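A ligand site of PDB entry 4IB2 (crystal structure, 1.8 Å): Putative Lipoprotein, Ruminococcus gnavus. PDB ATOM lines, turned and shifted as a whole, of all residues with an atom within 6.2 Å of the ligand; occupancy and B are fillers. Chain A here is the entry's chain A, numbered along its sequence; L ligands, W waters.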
ATOM      1  N   SER A  18      15.318   9.931  25.321  1.00  0.00           N
ATOM      2  CA  SER A  18      14.366  10.076  24.224  1.00  0.00           C
ATOM      3  C   SER A  18      14.353  11.536  23.786  1.00  0.00           C
ATOM      4  O   SER A  18      14.719  12.416  24.582  1.00  0.00           O
ATOM      5  CB  SER A  18      12.961   9.640  24.650  1.00  0.00           C
ATOM      6  OG  SER A  18      12.896   8.248  24.891  1.00  0.00           O
ATOM      7  N   PRO A  21       9.586  14.027  25.692  1.00  0.00           N
ATOM      8  CA  PRO A  21      10.023  15.264  26.357  1.00  0.00           C
ATOM      9  C   PRO A  21      11.440  15.203  26.943  1.00  0.00           C
ATOM     10  O   PRO A  21      11.964  16.234  27.332  1.00  0.00           O
ATOM     11  CB  PRO A  21       9.014  15.374  27.522  1.00  0.00           C
ATOM     12  CG  PRO A  21       8.747  13.937  27.908  1.00  0.00           C
ATOM     13  CD  PRO A  21       8.716  13.206  26.572  1.00  0.00           C
ATOM     14  N   HIS A  22      11.988  14.003  27.129  1.00  0.00           N
ATOM     15  CA  HIS A  22      13.209  13.711  27.912  1.00  0.00           C
ATOM     16  C   HIS A  22      14.391  14.623  27.597  1.00  0.00           C
ATOM     17  O   HIS A  22      14.867  15.303  28.511  1.00  0.00           O
ATOM     18  CB  HIS A  22      13.611  12.240  27.818  1.00  0.00           C
ATOM     19  CG  HIS A  22      12.488  11.310  28.149  1.00  0.00           C
ATOM     20  ND1 HIS A  22      11.372  11.228  27.338  1.00  0.00           N
ATOM     21  CD2 HIS A  22      12.260  10.585  29.277  1.00  0.00           C
ATOM     22  CE1 HIS A  22      10.554  10.384  27.934  1.00  0.00           C
ATOM     23  NE2 HIS A  22      11.036   9.974  29.108  1.00  0.00           N
ATOM     24  N   TYR A  48      14.091   2.157  22.273  1.00  0.00           N
ATOM     25  CA  TYR A  48      13.966   1.798  23.701  1.00  0.00           C
ATOM     26  C   TYR A  48      15.019   0.789  24.153  1.00  0.00           C
ATOM     27  O   TYR A  48      14.984   0.367  25.312  1.00  0.00           O
ATOM     28  CB  TYR A  48      12.559   1.208  23.942  1.00  0.00           C
ATOM     29  CG  TYR A  48      11.411   2.185  24.038  1.00  0.00           C
ATOM     30  CD1 TYR A  48      11.636   3.555  24.201  1.00  0.00           C
ATOM     31  CD2 TYR A  48      10.082   1.741  24.084  1.00  0.00           C
ATOM     32  CE1 TYR A  48      10.573   4.454  24.362  1.00  0.00           C
ATOM     33  CE2 TYR A  48       9.026   2.621  24.286  1.00  0.00           C
ATOM     34  CZ  TYR A  48       9.274   3.969  24.418  1.00  0.00           C
ATOM     35  OH  TYR A  48       8.195   4.815  24.537  1.00  0.00           O
ATOM     36  N   PHE A  65      14.484   7.715  29.857  1.00  0.00           N
ATOM     37  CA  PHE A  65      13.595   7.336  28.741  1.00  0.00           C
ATOM     38  C   PHE A  65      12.544   6.301  29.114  1.00  0.00           C
ATOM     39  O   PHE A  65      11.617   6.158  28.344  1.00  0.00           O
ATOM     40  CB  PHE A  65      14.433   6.727  27.555  1.00  0.00           C
ATOM     41  CG  PHE A  65      14.788   5.261  27.732  1.00  0.00           C
ATOM     42  CD1 PHE A  65      15.768   4.855  28.627  1.00  0.00           C
ATOM     43  CD2 PHE A  65      14.111   4.280  27.005  1.00  0.00           C
ATOM     44  CE1 PHE A  65      16.080   3.510  28.798  1.00  0.00           C
ATOM     45  CE2 PHE A  65      14.420   2.923  27.182  1.00  0.00           C
ATOM     46  CZ  PHE A  65      15.417   2.553  28.060  1.00  0.00           C
ATOM     47  N   GLN A  66      12.716   5.536  30.201  1.00  0.00           N
ATOM     48  CA  GLN A  66      11.850   4.391  30.513  1.00  0.00           C
ATOM     49  C   GLN A  66      11.122   4.484  31.842  1.00  0.00           C
ATOM     50  O   GLN A  66      11.481   5.272  32.720  1.00  0.00           O
ATOM     51  CB  GLN A  66      12.732   3.128  30.551  1.00  0.00           C
ATOM     52  CG  GLN A  66      13.513   2.941  31.882  1.00  0.00           C
ATOM     53  CD  GLN A  66      14.656   2.005  31.740  1.00  0.00           C
ATOM     54  OE1 GLN A  66      14.508   0.839  31.353  1.00  0.00           O
ATOM     55  NE2 GLN A  66      15.858   2.499  32.002  1.00  0.00           N
ATOM     56  N   HIS A  67      10.079   3.659  31.977  1.00  0.00           N
ATOM     57  CA  HIS A  67       9.342   3.552  33.228  1.00  0.00           C
ATOM     58  C   HIS A  67       9.844   2.338  33.997  1.00  0.00           C
ATOM     59  O   HIS A  67      10.608   1.534  33.456  1.00  0.00           O
ATOM     60  CB  HIS A  67       7.797   3.564  33.021  1.00  0.00           C
ATOM     61  CG  HIS A  67       7.266   2.618  31.983  1.00  0.00           C
ATOM     62  ND1 HIS A  67       7.505   1.251  32.034  1.00  0.00           N
ATOM     63  CD2 HIS A  67       6.536   2.892  30.880  1.00  0.00           C
ATOM     64  CE1 HIS A  67       6.880   0.739  30.990  1.00  0.00           C
ATOM     65  NE2 HIS A  67       6.310   1.692  30.247  1.00  0.00           N
ATOM     66  N   TYR A  70       9.225  -1.237  32.598  1.00  0.00           N
ATOM     67  CA  TYR A  70      10.117  -1.461  31.469  1.00  0.00           C
ATOM     68  C   TYR A  70      11.527  -1.829  31.949  1.00  0.00           C
ATOM     69  O   TYR A  70      12.113  -2.773  31.438  1.00  0.00           O
ATOM     70  CB  TYR A  70      10.215  -0.240  30.547  1.00  0.00           C
ATOM     71  CG  TYR A  70      10.988  -0.550  29.286  1.00  0.00           C
ATOM     72  CD1 TYR A  70      12.385  -0.419  29.247  1.00  0.00           C
ATOM     73  CD2 TYR A  70      10.344  -1.021  28.147  1.00  0.00           C
ATOM     74  CE1 TYR A  70      13.107  -0.708  28.094  1.00  0.00           C
ATOM     75  CE2 TYR A  70      11.058  -1.329  26.987  1.00  0.00           C
ATOM     76  CZ  TYR A  70      12.445  -1.196  26.977  1.00  0.00           C
ATOM     77  OH  TYR A  70      13.156  -1.523  25.854  1.00  0.00           O
ATOM     78  N   HIS A  89       8.602  11.598  36.039  1.00  0.00           N
ATOM     79  CA  HIS A  89       7.369  12.090  35.416  1.00  0.00           C
ATOM     80  C   HIS A  89       6.566  10.962  34.867  1.00  0.00           C
ATOM     81  O   HIS A  89       7.083   9.871  34.697  1.00  0.00           O
ATOM     82  CB  HIS A  89       7.712  13.108  34.277  1.00  0.00           C
ATOM     83  CG  HIS A  89       8.209  12.482  33.006  1.00  0.00           C
ATOM     84  ND1 HIS A  89       9.573  12.423  32.696  1.00  0.00           N
ATOM     85  CD2 HIS A  89       7.513  11.857  32.017  1.00  0.00           C
ATOM     86  CE1 HIS A  89       9.652  11.824  31.512  1.00  0.00           C
ATOM     87  NE2 HIS A  89       8.433  11.437  31.087  1.00  0.00           N
ATOM     88  N   TYR A  90       5.309  11.249  34.498  1.00  0.00           N
ATOM     89  CA  TYR A  90       4.445  10.231  33.934  1.00  0.00           C
ATOM     90  C   TYR A  90       3.837  10.746  32.600  1.00  0.00           C
ATOM     91  O   TYR A  90       3.625  11.958  32.430  1.00  0.00           O
ATOM     92  CB  TYR A  90       3.366   9.836  34.972  1.00  0.00           C
ATOM     93  CG  TYR A  90       2.117   9.214  34.385  1.00  0.00           C
ATOM     94  CD1 TYR A  90       2.140   7.930  33.831  1.00  0.00           C
ATOM     95  CD2 TYR A  90       0.928   9.934  34.321  1.00  0.00           C
ATOM     96  CE1 TYR A  90       1.005   7.371  33.248  1.00  0.00           C
ATOM     97  CE2 TYR A  90      -0.225   9.381  33.754  1.00  0.00           C
ATOM     98  CZ  TYR A  90      -0.179   8.092  33.229  1.00  0.00           C
ATOM     99  OH  TYR A  90      -1.316   7.568  32.676  1.00  0.00           O
ATOM    100  N   GLU A  91       3.674   9.845  31.631  1.00  0.00           N
ATOM    101  CA  GLU A  91       3.103  10.182  30.329  1.00  0.00           C
ATOM    102  C   GLU A  91       1.823   9.412  30.064  1.00  0.00           C
ATOM    103  O   GLU A  91       1.918   8.206  29.744  1.00  0.00           O
ATOM    104  CB  GLU A  91       4.080   9.880  29.177  1.00  0.00           C
ATOM    105  CG  GLU A  91       5.353  10.711  29.170  1.00  0.00           C
ATOM    106  CD  GLU A  91       6.455  10.169  28.274  1.00  0.00           C
ATOM    107  OE1 GLU A  91       6.176   9.303  27.415  1.00  0.00           O
ATOM    108  OE2 GLU A  91       7.621  10.566  28.497  1.00  0.00           O
ATOM    109  N   PHE A  93      -0.703   7.245  28.359  1.00  0.00           N
ATOM    110  CA  PHE A  93      -0.713   6.367  27.178  1.00  0.00           C
ATOM    111  C   PHE A  93      -2.052   6.553  26.489  1.00  0.00           C
ATOM    112  O   PHE A  93      -3.054   6.723  27.168  1.00  0.00           O
ATOM    113  CB  PHE A  93      -0.564   4.919  27.679  1.00  0.00           C
ATOM    114  CG  PHE A  93       0.014   3.870  26.764  1.00  0.00           C
ATOM    115  CD1 PHE A  93       1.278   4.018  26.221  1.00  0.00           C
ATOM    116  CD2 PHE A  93      -0.647   2.662  26.586  1.00  0.00           C
ATOM    117  CE1 PHE A  93       1.835   3.012  25.420  1.00  0.00           C
ATOM    118  CE2 PHE A  93      -0.065   1.639  25.833  1.00  0.00           C
ATOM    119  CZ  PHE A  93       1.149   1.839  25.219  1.00  0.00           C
ATOM    120  N   ASP A 117       7.079  -4.512  23.111  1.00  0.00           N
ATOM    121  CA  ASP A 117       7.870  -4.920  24.288  1.00  0.00           C
ATOM    122  C   ASP A 117       6.883  -5.357  25.370  1.00  0.00           C
ATOM    123  O   ASP A 117       5.751  -4.867  25.397  1.00  0.00           O
ATOM    124  CB  ASP A 117       8.783  -3.785  24.769  1.00  0.00           C
ATOM    125  CG  ASP A 117       8.030  -2.531  25.105  1.00  0.00           C
ATOM    126  OD1 ASP A 117       7.595  -1.827  24.158  1.00  0.00           O
ATOM    127  OD2 ASP A 117       7.780  -2.307  26.313  1.00  0.00           O
ATOM    128  N   THR A 119       6.087  -4.831  28.666  1.00  0.00           N
ATOM    129  CA  THR A 119       5.288  -3.970  29.527  1.00  0.00           C
ATOM    130  C   THR A 119       4.477  -2.948  28.770  1.00  0.00           C
ATOM    131  O   THR A 119       3.380  -2.636  29.234  1.00  0.00           O
ATOM    132  CB  THR A 119       6.131  -3.336  30.639  1.00  0.00           C
ATOM    133  OG1 THR A 119       7.090  -2.451  30.061  1.00  0.00           O
ATOM    134  CG2 THR A 119       6.826  -4.387  31.510  1.00  0.00           C
ATOM    135  N   ASN A 120       4.972  -2.438  27.627  1.00  0.00           N
ATOM    136  CA  ASN A 120       4.163  -1.476  26.866  1.00  0.00           C
ATOM    137  C   ASN A 120       3.067  -2.179  26.072  1.00  0.00           C
ATOM    138  O   ASN A 120       1.984  -1.602  25.876  1.00  0.00           O
ATOM    139  CB  ASN A 120       5.051  -0.589  26.022  1.00  0.00           C
ATOM    140  CG  ASN A 120       5.801   0.397  26.897  1.00  0.00           C
ATOM    141  OD1 ASN A 120       5.200   1.158  27.661  1.00  0.00           O
ATOM    142  ND2 ASN A 120       7.128   0.272  26.951  1.00  0.00           N
ATOM    143  N   ARG A 123       0.510  -2.850  28.704  1.00  0.00           N
ATOM    144  CA  ARG A 123      -0.121  -1.545  28.966  1.00  0.00           C
ATOM    145  C   ARG A 123      -1.202  -1.217  27.915  1.00  0.00           C
ATOM    146  O   ARG A 123      -2.276  -0.705  28.276  1.00  0.00           O
ATOM    147  CB  ARG A 123       0.950  -0.473  28.939  1.00  0.00           C
ATOM    148  CG  ARG A 123       0.483   0.877  29.448  1.00  0.00           C
ATOM    149  CD  ARG A 123       1.683   1.788  29.371  1.00  0.00           C
ATOM    150  NE  ARG A 123       1.380   3.110  29.899  1.00  0.00           N
ATOM    151  CZ  ARG A 123       2.278   4.082  30.002  1.00  0.00           C
ATOM    152  NH1 ARG A 123       3.516   3.907  29.549  1.00  0.00           N
ATOM    153  NH2 ARG A 123       1.937   5.235  30.526  1.00  0.00           N
ATOM    154  N   ASN A 179       3.009   5.489  23.030  1.00  0.00           N
ATOM    155  CA  ASN A 179       3.675   6.002  24.221  1.00  0.00           C
ATOM    156  C   ASN A 179       3.703   7.503  24.073  1.00  0.00           C
ATOM    157  O   ASN A 179       3.873   7.984  22.947  1.00  0.00           O
ATOM    158  CB  ASN A 179       5.139   5.451  24.309  1.00  0.00           C
ATOM    159  CG  ASN A 179       5.186   3.998  24.597  1.00  0.00           C
ATOM    160  OD1 ASN A 179       5.210   3.143  23.697  1.00  0.00           O
ATOM    161  ND2 ASN A 179       5.175   3.673  25.888  1.00  0.00           N
ATOM    162  N   GLY A 180       3.482   8.220  25.171  1.00  0.00           N
ATOM    163  CA  GLY A 180       3.517   9.693  25.149  1.00  0.00           C
ATOM    164  C   GLY A 180       4.695  10.311  24.404  1.00  0.00           C
ATOM    165  O   GLY A 180       4.527  11.211  23.585  1.00  0.00           O
ATOM    166  N   ASN A 181       5.908   9.850  24.700  1.00  0.00           N
ATOM    167  CA  ASN A 181       7.111  10.394  24.064  1.00  0.00           C
ATOM    168  C   ASN A 181       7.049  10.255  22.513  1.00  0.00           C
ATOM    169  O   ASN A 181       7.434  11.178  21.813  1.00  0.00           O
ATOM    170  CB  ASN A 181       8.379   9.722  24.631  1.00  0.00           C
ATOM    171  CG  ASN A 181       8.660   8.335  24.110  1.00  0.00           C
ATOM    172  OD1 ASN A 181       8.053   7.354  24.549  1.00  0.00           O
ATOM    173  ND2 ASN A 181       9.572   8.229  23.152  1.00  0.00           N
ATOM    174  N   TYR A 208       3.610   3.689  35.679  1.00  0.00           N
ATOM    175  CA  TYR A 208       4.517   3.949  34.564  1.00  0.00           C
ATOM    176  C   TYR A 208       5.243   5.279  34.733  1.00  0.00           C
ATOM    177  O   TYR A 208       5.313   6.076  33.798  1.00  0.00           O
ATOM    178  CB  TYR A 208       3.727   3.905  33.245  1.00  0.00           C
ATOM    179  CG  TYR A 208       3.034   2.568  33.075  1.00  0.00           C
ATOM    180  CD1 TYR A 208       3.771   1.404  32.835  1.00  0.00           C
ATOM    181  CD2 TYR A 208       1.653   2.472  33.152  1.00  0.00           C
ATOM    182  CE1 TYR A 208       3.124   0.180  32.646  1.00  0.00           C
ATOM    183  CE2 TYR A 208       1.009   1.237  33.016  1.00  0.00           C
ATOM    184  CZ  TYR A 208       1.747   0.094  32.770  1.00  0.00           C
ATOM    185  OH  TYR A 208       1.077  -1.082  32.586  1.00  0.00           O
ATOM    186  N   VAL A 209       5.949   5.417  35.871  1.00  0.00           N
ATOM    187  CA  VAL A 209       6.697   6.646  36.131  1.00  0.00           C
ATOM    188  C   VAL A 209       8.031   6.542  35.415  1.00  0.00           C
ATOM    189  O   VAL A 209       8.690   5.507  35.520  1.00  0.00           O
ATOM    190  CB  VAL A 209       6.834   6.946  37.643  1.00  0.00           C
ATOM    191  CG1 VAL A 209       7.372   5.729  38.403  1.00  0.00           C
ATOM    192  CG2 VAL A 209       7.730   8.166  37.878  1.00  0.00           C
ATOM    193  N   ASN A 210       8.416   7.608  34.676  1.00  0.00           N
ATOM    194  CA  ASN A 210       9.719   7.651  33.977  1.00  0.00           C
ATOM    195  C   ASN A 210      10.798   7.978  34.960  1.00  0.00           C
ATOM    196  O   ASN A 210      10.627   8.808  35.855  1.00  0.00           O
ATOM    197  CB  ASN A 210       9.729   8.613  32.789  1.00  0.00           C
ATOM    198  CG  ASN A 210       8.985   8.047  31.611  1.00  0.00           C
ATOM    199  OD1 ASN A 210       9.476   8.088  30.484  1.00  0.00           O
ATOM    200  ND2 ASN A 210       7.758   7.504  31.821  1.00  0.00           N
HETATM  201  N1  LIG L   1       8.210   7.616  27.825  1.00  0.00           N
HETATM  202  C1  LIG L   1       7.621   6.241  27.693  1.00  0.00           C
HETATM  203  C2  LIG L   1       6.295   6.205  28.485  1.00  0.00           C
HETATM  204  O1  LIG L   1       6.241   6.840  29.568  1.00  0.00           O
HETATM  205  C3  LIG L   1       8.584   5.175  28.219  1.00  0.00           C
HETATM  206  C4  LIG L   1       8.122   3.707  27.923  1.00  0.00           C
HETATM  207  S1  LIG L   1       9.182   2.430  28.603  1.00  0.00           S
HETATM  208  C5  LIG L   1      10.685   2.633  27.525  1.00  0.00           C
HETATM  209  O2  LIG L   1       5.311   5.576  28.015  1.00  0.00           O
HETATM  210  O   HOH W   1       2.856   6.774  27.508  1.00  0.00           O
HETATM  211  O   HOH W   2       4.280   6.963  31.400  1.00  0.00           O
HETATM  212  O   HOH W   3      10.730   7.402  26.303  1.00  0.00           O
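Residues that only touch the ligand: Phe 65 (3.2 Å), Tyr 70 (3.5 Å), Tyr 48 (3.5 Å), His 22 (3.6 Å) and Gln 66 (3.7 Å). Hydrophobic or aromatic side chains that line the ligand: His 22, Tyr 48, Phe 65, His 67 and Tyr 70. Within 4 Å of the ligand: His 22, Tyr 48, Phe 65, Gln 66, His 67, Tyr 70, Glu 91, Asn 120, Arg 123, Asn 179, Asn 181 and Asn 210. The nearest printed residue that does not touch the ligand is Gly 180 (4.3 Å).
N1 of the ligand is in salt-bridge range of OE1 of Glu 91. O1 of the ligand is in hydrogen-bond range of ND2 of Asn 210. The side-chain amide nitrogen (ND2) of Asn 179 lies within hydrogen-bond range of an oxygen (O2) of the ligand (2.9 Å). An oxygen (O2) of the ligand is in salt-bridge range of the guanidinium group of Arg 123 (2.9 Å). The side-chain amide oxygen (OD1) of Asn 181 is in hydrogen-bond range of a nitrogen (N1) of the ligand (3.3 Å). N of His 67 sits close to S1 of the ligand, 3.7 Å away. NE2 of His 67 sits close to S1 of the ligand (3.4 Å). ND2 of Asn 120 sits close to S1 of the ligand, 3.4 Å away.
Water W2 lies within hydrogen-bond range of O1 of the ligand (2.7 Å), O of Tyr 208 (2.8 Å), N of Glu 91 (3.0 Å) and NH2 of Arg 123 (3.0 Å). Water W1 lies within hydrogen-bond range of O2 of the ligand (2.8 Å), O of Glu 91 (2.8 Å) and N of Gly 180 (2.8 Å). Water W3 lies within hydrogen-bond range of the backbone carbonyl oxygen (O) of Phe 65 (2.5 Å), the side-chain hydroxyl (OG) of Ser 18 (2.7 Å), a nitrogen (N1) of the ligand (3.0 Å) and the side-chain amide oxygen (OD1) of Asn 181 (3.2 Å).
The backbone carbonyl oxygen of Glu 91 is in hydrogen-bond range of the guanidinium group of Arg 123, at 3.1 Å. The side-chain carboxylate (OE2) of Glu 91 is in hydrogen-bond range of a ring nitrogen (NE2) of His 89 (2.9 Å). A ring nitrogen (NE2) of His 22 is in hydrogen-bond range of the side-chain amide oxygen of Asn 210 (2.8 Å). O of Tyr 208 sits at hydrogen-bond distance from ND2 of Asn 210 (3.5 Å). A ring nitrogen (NE2) of His 67 is in hydrogen-bond range of the side-chain amide oxygen of Asn 120, 2.9 Å away. N of Tyr 70 lies within hydrogen-bond range of ND1 of His 67 (3.1 Å). ND2 of Asn 120 is in hydrogen-bond range of OD2 of Asp 117, 2.7 Å away. The side-chain hydroxyl of Tyr 70 sits at hydrogen-bond distance from the backbone carbonyl oxygen of Tyr 48 (2.7 Å).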
